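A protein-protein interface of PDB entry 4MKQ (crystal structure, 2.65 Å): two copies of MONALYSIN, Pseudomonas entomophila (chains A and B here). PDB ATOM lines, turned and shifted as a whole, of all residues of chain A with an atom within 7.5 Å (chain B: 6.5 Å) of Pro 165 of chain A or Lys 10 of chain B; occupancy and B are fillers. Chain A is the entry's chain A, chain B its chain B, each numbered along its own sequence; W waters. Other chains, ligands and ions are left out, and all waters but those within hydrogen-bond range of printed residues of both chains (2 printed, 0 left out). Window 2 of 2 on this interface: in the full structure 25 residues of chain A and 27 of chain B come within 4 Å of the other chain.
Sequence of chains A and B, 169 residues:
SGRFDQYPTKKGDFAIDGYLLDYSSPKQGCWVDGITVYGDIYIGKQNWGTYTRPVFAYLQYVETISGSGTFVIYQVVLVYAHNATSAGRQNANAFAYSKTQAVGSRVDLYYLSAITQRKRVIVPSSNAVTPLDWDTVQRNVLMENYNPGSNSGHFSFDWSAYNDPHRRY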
ATOM      1  N   VAL A  37      10.449 -20.847  25.662  1.00  0.00           N
ATOM      2  CA  VAL A  37      11.260 -19.649  25.881  1.00  0.00           C
ATOM      3  C   VAL A  37      12.737 -20.026  25.785  1.00  0.00           C
ATOM      4  O   VAL A  37      13.054 -21.213  25.786  1.00  0.00           O
ATOM      5  CB  VAL A  37      10.924 -18.916  27.216  1.00  0.00           C
ATOM      6  CG1 VAL A  37       9.490 -18.413  27.223  1.00  0.00           C
ATOM      7  CG2 VAL A  37      11.199 -19.791  28.434  1.00  0.00           C
ATOM      8  N   TYR A  38      13.632 -19.030  25.715  1.00  0.00           N
ATOM      9  CA  TYR A  38      15.074 -19.265  25.648  1.00  0.00           C
ATOM     10  C   TYR A  38      15.845 -18.247  26.483  1.00  0.00           C
ATOM     11  O   TYR A  38      15.596 -17.048  26.391  1.00  0.00           O
ATOM     12  CB  TYR A  38      15.563 -19.304  24.190  1.00  0.00           C
ATOM     13  CG  TYR A  38      17.034 -19.627  24.043  1.00  0.00           C
ATOM     14  CD1 TYR A  38      17.480 -20.944  24.011  1.00  0.00           C
ATOM     15  CD2 TYR A  38      17.978 -18.616  23.919  1.00  0.00           C
ATOM     16  CE1 TYR A  38      18.835 -21.246  23.876  1.00  0.00           C
ATOM     17  CE2 TYR A  38      19.332 -18.906  23.785  1.00  0.00           C
ATOM     18  CZ  TYR A  38      19.759 -20.221  23.764  1.00  0.00           C
ATOM     19  OH  TYR A  38      21.099 -20.496  23.620  1.00  0.00           O
ATOM     20  N   SER A 160      11.905 -21.890  17.758  1.00  0.00           N
ATOM     21  CA  SER A 160      11.769 -20.512  17.254  1.00  0.00           C
ATOM     22  C   SER A 160      11.931 -19.460  18.361  1.00  0.00           C
ATOM     23  O   SER A 160      12.170 -18.288  18.061  1.00  0.00           O
ATOM     24  CB  SER A 160      10.450 -20.324  16.509  1.00  0.00           C
ATOM     25  OG  SER A 160       9.346 -20.210  17.392  1.00  0.00           O
ATOM     26  N   ALA A 161      11.828 -19.899  19.642  1.00  0.00           N
ATOM     27  CA  ALA A 161      12.007 -19.097  20.857  1.00  0.00           C
ATOM     28  C   ALA A 161      13.316 -18.311  20.808  1.00  0.00           C
ATOM     29  O   ALA A 161      13.342 -17.151  21.202  1.00  0.00           O
ATOM     30  CB  ALA A 161      11.997 -20.004  22.074  1.00  0.00           C
ATOM     31  N   TYR A 162      14.383 -18.940  20.266  1.00  0.00           N
ATOM     32  CA  TYR A 162      15.725 -18.382  20.073  1.00  0.00           C
ATOM     33  C   TYR A 162      15.687 -17.102  19.226  1.00  0.00           C
ATOM     34  O   TYR A 162      16.550 -16.242  19.391  1.00  0.00           O
ATOM     35  CB  TYR A 162      16.630 -19.435  19.393  1.00  0.00           C
ATOM     36  CG  TYR A 162      18.101 -19.071  19.353  1.00  0.00           C
ATOM     37  CD1 TYR A 162      18.638 -18.364  18.277  1.00  0.00           C
ATOM     38  CD2 TYR A 162      18.965 -19.464  20.370  1.00  0.00           C
ATOM     39  CE1 TYR A 162      19.987 -18.014  18.243  1.00  0.00           C
ATOM     40  CE2 TYR A 162      20.318 -19.128  20.341  1.00  0.00           C
ATOM     41  CZ  TYR A 162      20.826 -18.407  19.273  1.00  0.00           C
ATOM     42  OH  TYR A 162      22.161 -18.082  19.239  1.00  0.00           O
ATOM     43  N   ASN A 163      14.705 -16.986  18.316  1.00  0.00           N
ATOM     44  CA  ASN A 163      14.585 -15.837  17.414  1.00  0.00           C
ATOM     45  C   ASN A 163      13.485 -14.832  17.813  1.00  0.00           C
ATOM     46  O   ASN A 163      13.359 -13.787  17.167  1.00  0.00           O
ATOM     47  CB  ASN A 163      14.417 -16.318  15.970  1.00  0.00           C
ATOM     48  CG  ASN A 163      15.579 -17.156  15.486  1.00  0.00           C
ATOM     49  OD1 ASN A 163      16.743 -16.727  15.511  1.00  0.00           O
ATOM     50  ND2 ASN A 163      15.290 -18.382  15.055  1.00  0.00           N
ATOM     51  N   ASP A 164      12.714 -15.125  18.887  1.00  0.00           N
ATOM     52  CA  ASP A 164      11.670 -14.224  19.379  1.00  0.00           C
ATOM     53  C   ASP A 164      12.196 -13.442  20.591  1.00  0.00           C
ATOM     54  O   ASP A 164      12.446 -14.051  21.632  1.00  0.00           O
ATOM     55  CB  ASP A 164      10.372 -14.987  19.724  1.00  0.00           C
ATOM     56  CG  ASP A 164       9.139 -14.120  19.949  1.00  0.00           C
ATOM     57  OD1 ASP A 164       9.284 -12.883  20.035  1.00  0.00           O
ATOM     58  OD2 ASP A 164       8.026 -14.679  20.019  1.00  0.00           O
ATOM     59  N   PRO A 165      12.365 -12.098  20.486  1.00  0.00           N
ATOM     60  CA  PRO A 165      12.858 -11.322  21.641  1.00  0.00           C
ATOM     61  C   PRO A 165      11.905 -11.321  22.840  1.00  0.00           C
ATOM     62  O   PRO A 165      12.355 -11.127  23.969  1.00  0.00           O
ATOM     63  CB  PRO A 165      13.043  -9.907  21.073  1.00  0.00           C
ATOM     64  CG  PRO A 165      13.018 -10.062  19.594  1.00  0.00           C
ATOM     65  CD  PRO A 165      12.122 -11.222  19.325  1.00  0.00           C
ATOM     66  N   HIS A 166      10.597 -11.558  22.591  1.00  0.00           N
ATOM     67  CA  HIS A 166       9.534 -11.630  23.599  1.00  0.00           C
ATOM     68  C   HIS A 166       9.702 -12.877  24.454  1.00  0.00           C
ATOM     69  O   HIS A 166       9.331 -12.865  25.627  1.00  0.00           O
ATOM     70  CB  HIS A 166       8.151 -11.682  22.919  1.00  0.00           C
ATOM     71  CG  HIS A 166       7.718 -10.425  22.222  1.00  0.00           C
ATOM     72  ND1 HIS A 166       6.375 -10.149  22.017  1.00  0.00           N
ATOM     73  CD2 HIS A 166       8.453  -9.421  21.686  1.00  0.00           C
ATOM     74  CE1 HIS A 166       6.338  -8.991  21.379  1.00  0.00           C
ATOM     75  NE2 HIS A 166       7.563  -8.511  21.165  1.00  0.00           N
ATOM     76  N   ARG A 167      10.237 -13.961  23.852  1.00  0.00           N
ATOM     77  CA  ARG A 167      10.466 -15.260  24.485  1.00  0.00           C
ATOM     78  C   ARG A 167      11.937 -15.488  24.861  1.00  0.00           C
ATOM     79  O   ARG A 167      12.331 -16.616  25.158  1.00  0.00           O
ATOM     80  CB  ARG A 167       9.925 -16.387  23.594  1.00  0.00           C
ATOM     81  CG  ARG A 167       8.406 -16.508  23.638  1.00  0.00           C
ATOM     82  CD  ARG A 167       7.818 -16.910  22.299  1.00  0.00           C
ATOM     83  NE  ARG A 167       8.115 -18.298  21.953  1.00  0.00           N
ATOM     84  CZ  ARG A 167       8.398 -18.727  20.728  1.00  0.00           C
ATOM     85  NH1 ARG A 167       8.440 -17.877  19.710  1.00  0.00           N
ATOM     86  NH2 ARG A 167       8.655 -20.009  20.512  1.00  0.00           N
ATOM     87  N   ARG A 168      12.743 -14.410  24.875  1.00  0.00           N
ATOM     88  CA  ARG A 168      14.157 -14.453  25.251  1.00  0.00           C
ATOM     89  C   ARG A 168      14.391 -13.617  26.499  1.00  0.00           C
ATOM     90  O   ARG A 168      13.689 -12.627  26.703  1.00  0.00           O
ATOM     91  CB  ARG A 168      15.054 -13.967  24.107  1.00  0.00           C
ATOM     92  CG  ARG A 168      15.343 -15.023  23.053  1.00  0.00           C
ATOM     93  CD  ARG A 168      16.521 -14.621  22.187  1.00  0.00           C
ATOM     94  NE  ARG A 168      17.806 -14.880  22.845  1.00  0.00           N
ATOM     95  CZ  ARG A 168      18.867 -15.414  22.247  1.00  0.00           C
ATOM     96  NH1 ARG A 168      18.814 -15.759  20.966  1.00  0.00           N
ATOM     97  NH2 ARG A 168      19.989 -15.611  22.926  1.00  0.00           N
ATOM     98  N   TYR A 169      15.369 -14.010  27.339  1.00  0.00           N
ATOM     99  CA  TYR A 169      15.681 -13.285  28.575  1.00  0.00           C
ATOM    100  C   TYR A 169      17.164 -13.319  28.938  1.00  0.00           C
ATOM    101  O   TYR A 169      17.854 -14.290  28.637  1.00  0.00           O
ATOM    102  CB  TYR A 169      14.795 -13.774  29.737  1.00  0.00           C
ATOM    103  CG  TYR A 169      15.015 -15.212  30.159  1.00  0.00           C
ATOM    104  CD1 TYR A 169      14.299 -16.251  29.568  1.00  0.00           C
ATOM    105  CD2 TYR A 169      15.882 -15.528  31.197  1.00  0.00           C
ATOM    106  CE1 TYR A 169      14.478 -17.572  29.974  1.00  0.00           C
ATOM    107  CE2 TYR A 169      16.060 -16.842  31.617  1.00  0.00           C
ATOM    108  CZ  TYR A 169      15.358 -17.861  31.000  1.00  0.00           C
ATOM    109  OH  TYR A 169      15.537 -19.156  31.411  1.00  0.00           O
ATOM    110  N   PRO B   8       8.760  -3.355  27.921  1.00  0.00           N
ATOM    111  CA  PRO B   8       8.681  -4.345  26.833  1.00  0.00           C
ATOM    112  C   PRO B   8       7.599  -5.393  27.057  1.00  0.00           C
ATOM    113  O   PRO B   8       6.997  -5.440  28.126  1.00  0.00           O
ATOM    114  CB  PRO B   8      10.073  -4.979  26.841  1.00  0.00           C
ATOM    115  CG  PRO B   8      10.501  -4.893  28.239  1.00  0.00           C
ATOM    116  CD  PRO B   8       9.913  -3.626  28.804  1.00  0.00           C
ATOM    117  N   THR B   9       7.361  -6.234  26.042  1.00  0.00           N
ATOM    118  CA  THR B   9       6.397  -7.326  26.094  1.00  0.00           C
ATOM    119  C   THR B   9       7.165  -8.644  26.244  1.00  0.00           C
ATOM    120  O   THR B   9       8.158  -8.867  25.543  1.00  0.00           O
ATOM    121  CB  THR B   9       5.484  -7.285  24.855  1.00  0.00           C
ATOM    122  OG1 THR B   9       4.822  -6.020  24.817  1.00  0.00           O
ATOM    123  CG2 THR B   9       4.443  -8.410  24.836  1.00  0.00           C
ATOM    124  N   LYS B  10       6.715  -9.501  27.175  1.00  0.00           N
ATOM    125  CA  LYS B  10       7.312 -10.815  27.410  1.00  0.00           C
ATOM    126  C   LYS B  10       6.261 -11.911  27.274  1.00  0.00           C
ATOM    127  O   LYS B  10       5.078 -11.665  27.519  1.00  0.00           O
ATOM    128  CB  LYS B  10       8.039 -10.880  28.771  1.00  0.00           C
ATOM    129  CG  LYS B  10       9.322 -10.045  28.855  1.00  0.00           C
ATOM    130  CD  LYS B  10      10.485 -10.644  28.062  1.00  0.00           C
ATOM    131  CE  LYS B  10      11.594  -9.644  27.874  1.00  0.00           C
ATOM    132  NZ  LYS B  10      12.579 -10.091  26.859  1.00  0.00           N
ATOM    133  N   LYS B  11       6.690 -13.110  26.851  1.00  0.00           N
ATOM    134  CA  LYS B  11       5.817 -14.260  26.634  1.00  0.00           C
ATOM    135  C   LYS B  11       6.481 -15.500  27.230  1.00  0.00           C
ATOM    136  O   LYS B  11       7.628 -15.794  26.900  1.00  0.00           O
ATOM    137  CB  LYS B  11       5.566 -14.432  25.122  1.00  0.00           C
ATOM    138  CG  LYS B  11       4.437 -15.385  24.752  1.00  0.00           C
ATOM    139  CD  LYS B  11       4.273 -15.462  23.244  1.00  0.00           C
ATOM    140  CE  LYS B  11       3.062 -16.265  22.839  1.00  0.00           C
ATOM    141  NZ  LYS B  11       2.992 -16.436  21.365  1.00  0.00           N
ATOM    142  N   GLY B  12       5.763 -16.197  28.110  1.00  0.00           N
ATOM    143  CA  GLY B  12       6.254 -17.397  28.780  1.00  0.00           C
ATOM    144  C   GLY B  12       6.804 -17.114  30.161  1.00  0.00           C
ATOM    145  O   GLY B  12       7.555 -16.152  30.345  1.00  0.00           O
ATOM    146  N   ALA B  15      10.510 -16.297  30.759  1.00  0.00           N
ATOM    147  CA  ALA B  15      10.903 -15.048  30.089  1.00  0.00           C
ATOM    148  C   ALA B  15      10.477 -13.843  30.921  1.00  0.00           C
ATOM    149  O   ALA B  15      11.251 -12.897  31.057  1.00  0.00           O
ATOM    150  CB  ALA B  15      10.307 -14.971  28.695  1.00  0.00           C
ATOM    151  N   ILE B  16       9.265 -13.901  31.511  1.00  0.00           N
ATOM    152  CA  ILE B  16       8.701 -12.868  32.385  1.00  0.00           C
ATOM    153  C   ILE B  16       9.557 -12.765  33.660  1.00  0.00           C
ATOM    154  O   ILE B  16      10.007 -11.670  34.005  1.00  0.00           O
ATOM    155  CB  ILE B  16       7.198 -13.160  32.691  1.00  0.00           C
ATOM    156  CG1 ILE B  16       6.335 -13.063  31.415  1.00  0.00           C
ATOM    157  CG2 ILE B  16       6.657 -12.245  33.799  1.00  0.00           C
ATOM    158  CD1 ILE B  16       5.155 -13.994  31.391  1.00  0.00           C
ATOM    159  N   TYR B  19      13.312 -11.646  32.909  1.00  0.00           N
ATOM    160  CA  TYR B  19      13.431 -10.217  32.642  1.00  0.00           C
ATOM    161  C   TYR B  19      13.307  -9.380  33.924  1.00  0.00           C
ATOM    162  O   TYR B  19      14.126  -8.488  34.144  1.00  0.00           O
ATOM    163  CB  TYR B  19      12.406  -9.762  31.573  1.00  0.00           C
ATOM    164  CG  TYR B  19      12.349  -8.259  31.388  1.00  0.00           C
ATOM    165  CD1 TYR B  19      13.363  -7.581  30.716  1.00  0.00           C
ATOM    166  CD2 TYR B  19      11.301  -7.511  31.913  1.00  0.00           C
ATOM    167  CE1 TYR B  19      13.336  -6.194  30.577  1.00  0.00           C
ATOM    168  CE2 TYR B  19      11.264  -6.124  31.782  1.00  0.00           C
ATOM    169  CZ  TYR B  19      12.288  -5.469  31.118  1.00  0.00           C
ATOM    170  OH  TYR B  19      12.258  -4.103  30.982  1.00  0.00           O
ATOM    171  N   CYS B  30       6.657  -5.283  32.876  1.00  0.00           N
ATOM    172  CA  CYS B  30       6.624  -5.700  31.479  1.00  0.00           C
ATOM    173  C   CYS B  30       5.202  -6.099  31.106  1.00  0.00           C
ATOM    174  O   CYS B  30       4.445  -6.571  31.958  1.00  0.00           O
ATOM    175  CB  CYS B  30       7.620  -6.829  31.202  1.00  0.00           C
ATOM    176  SG  CYS B  30       7.162  -8.437  31.910  1.00  0.00           S
ATOM    177  N   TRP B  31       4.841  -5.891  29.842  1.00  0.00           N
ATOM    178  CA  TRP B  31       3.549  -6.301  29.307  1.00  0.00           C
ATOM    179  C   TRP B  31       3.634  -7.809  29.049  1.00  0.00           C
ATOM    180  O   TRP B  31       4.732  -8.331  28.828  1.00  0.00           O
ATOM    181  CB  TRP B  31       3.223  -5.523  28.024  1.00  0.00           C
ATOM    182  CG  TRP B  31       2.910  -4.077  28.277  1.00  0.00           C
ATOM    183  CD1 TRP B  31       3.778  -3.026  28.224  1.00  0.00           C
ATOM    184  CD2 TRP B  31       1.642  -3.533  28.665  1.00  0.00           C
ATOM    185  NE1 TRP B  31       3.123  -1.854  28.527  1.00  0.00           N
ATOM    186  CE2 TRP B  31       1.811  -2.137  28.808  1.00  0.00           C
ATOM    187  CE3 TRP B  31       0.370  -4.089  28.896  1.00  0.00           C
ATOM    188  CZ2 TRP B  31       0.762  -1.292  29.184  1.00  0.00           C
ATOM    189  CZ3 TRP B  31      -0.670  -3.246  29.260  1.00  0.00           C
ATOM    190  CH2 TRP B  31      -0.470  -1.867  29.398  1.00  0.00           C
ATOM    191  N   VAL B  32       2.507  -8.518  29.153  1.00  0.00           N
ATOM    192  CA  VAL B  32       2.506  -9.970  28.980  1.00  0.00           C
ATOM    193  C   VAL B  32       1.595 -10.404  27.843  1.00  0.00           C
ATOM    194  O   VAL B  32       0.410 -10.066  27.839  1.00  0.00           O
ATOM    195  CB  VAL B  32       2.189 -10.727  30.312  1.00  0.00           C
ATOM    196  CG1 VAL B  32       2.100 -12.237  30.100  1.00  0.00           C
ATOM    197  CG2 VAL B  32       3.214 -10.408  31.395  1.00  0.00           C
ATOM    198  N   ASP B  33       2.153 -11.164  26.882  1.00  0.00           N
ATOM    199  CA  ASP B  33       1.390 -11.758  25.785  1.00  0.00           C
ATOM    200  C   ASP B  33       1.033 -13.161  26.282  1.00  0.00           C
ATOM    201  O   ASP B  33       1.923 -13.976  26.538  1.00  0.00           O
ATOM    202  CB  ASP B  33       2.206 -11.802  24.475  1.00  0.00           C
ATOM    203  CG  ASP B  33       1.453 -12.306  23.250  1.00  0.00           C
ATOM    204  OD1 ASP B  33       0.199 -12.392  23.306  1.00  0.00           O
ATOM    205  OD2 ASP B  33       2.112 -12.581  22.222  1.00  0.00           O
ATOM    206  N   GLY B  34      -0.255 -13.385  26.512  1.00  0.00           N
ATOM    207  CA  GLY B  34      -0.744 -14.643  27.053  1.00  0.00           C
ATOM    208  C   GLY B  34      -2.018 -15.174  26.441  1.00  0.00           C
ATOM    209  O   GLY B  34      -2.704 -14.477  25.688  1.00  0.00           O
HETATM  210  O   HOH W   1      10.825  -8.615  24.772  1.00  0.00           O
HETATM  211  O   HOH W   2      14.891 -10.100  24.419  1.00  0.00           O
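The side-chain hydroxyl (OG) of Ser 160 of chain A is in hydrogen-bond range of the guanidinium group (NH2) of Arg 167 of chain A, at 3.2 Å.
The backbone carbonyl oxygen (O) of Tyr 162 of chain A is in hydrogen-bond range of the guanidinium group (NH1) of Arg 168 of chain A (2.8 Å).
The side-chain carboxylate (OD1) of Asp 164 of chain A sits at hydrogen-bond distance from the backbone NH (N) of His 166 of chain A, at 3.2 Å.
OD2 of Asp 164 of chain A is in salt-bridge range of NH1 of Arg 167 of chain A (3.2 Å).
The backbone NH of Lys 10 of chain B is in hydrogen-bond range of the backbone carbonyl oxygen of Trp 31 of chain B, 2.8 Å away.
N of Asp 33 of chain B is in hydrogen-bond range of O of Lys 10 of chain B, 3.0 Å away.
No position is printed for both chains.
CG1 of Val 37 of chain A touches O of Lys 11 of chain B, at 3.2 Å.
Val 37 of chain A touches Gly 12 of chain B.
Val 37 of chain A touches Ala 15 of chain B (CG1 to CB, 3.8 Å).
CA of His 166 of chain A touches O of Thr 9 of chain B (3.6 Å).
Lys 10 of chain B touches His 166 of chain A (CA to O, 3.4 Å).
His 166 of chain A touches Ala 15 of chain B.
CG of Arg 167 of chain A touches O of Lys 11 of chain B (3.4 Å).
Ala 15 of chain B touches Tyr 169 of chain A (CA to CD1, 3.6 Å).
Pro 165 of chain A touches just one residue of chain B: Lys 10.
Printed residues of chain A within 4 Å of Lys 10 of chain B: Pro 165, His 166 and Arg 168.
Of the printed residues of chain B, Val 37 of chain A touches Lys 11, Gly 12 and Ala 15.
Printed residues of chain B within 4 Å of Tyr 169 of chain A: Ala 15 (3.6 Å).
Of the printed residues of chain B, Arg 168 of chain A touches Lys 10 (2.8 Å).
Of the printed residues of chain A, Gly 12 of chain B touches Val 37 (3.7 Å).
The nearest residue of chain A that does not touch Lys 10 of chain B is Tyr 169 of chain A (4.8 Å).
The backbone carbonyl oxygen (O) of Pro 165 of chain A sits at hydrogen-bond distance from the side-chain amino group (NZ) of Lys 10 of chain B (3.1 Å).
N of Lys 11 of chain B sits at hydrogen-bond distance from O of His 166 of chain A.
The side-chain amino group (NZ) of Lys 10 of chain B is in hydrogen-bond range of the backbone carbonyl oxygen (O) of Arg 168 of chain A (2.8 Å).
Of the 12 printed residues of chain A, 6 touch a printed residue of chain B.
Printed residues of chain A that touch a printed residue of chain B: Val 37, Pro 165, His 166, Arg 167, Arg 168 and Tyr 169.
Hydrophobic or aromatic side chains of chain A that line the printed part of chain B: Val 37, His 166 and Tyr 169.
Of the 13 printed residues of chain B, 5 touch a printed residue of chain A.
Hydrophobic or aromatic side chains of chain B that line the printed part of chain A: Ala 15.
Water W2 bridges O of Pro 165 of chain A and NZ of Lys 10 of chain B.
Water W1 lies within hydrogen-bond range of O of Thr 9 of chain B (2.8 Å), O of Pro 165 of chain A (3.0 Å) and NZ of Lys 10 of chain B (3.1 Å).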
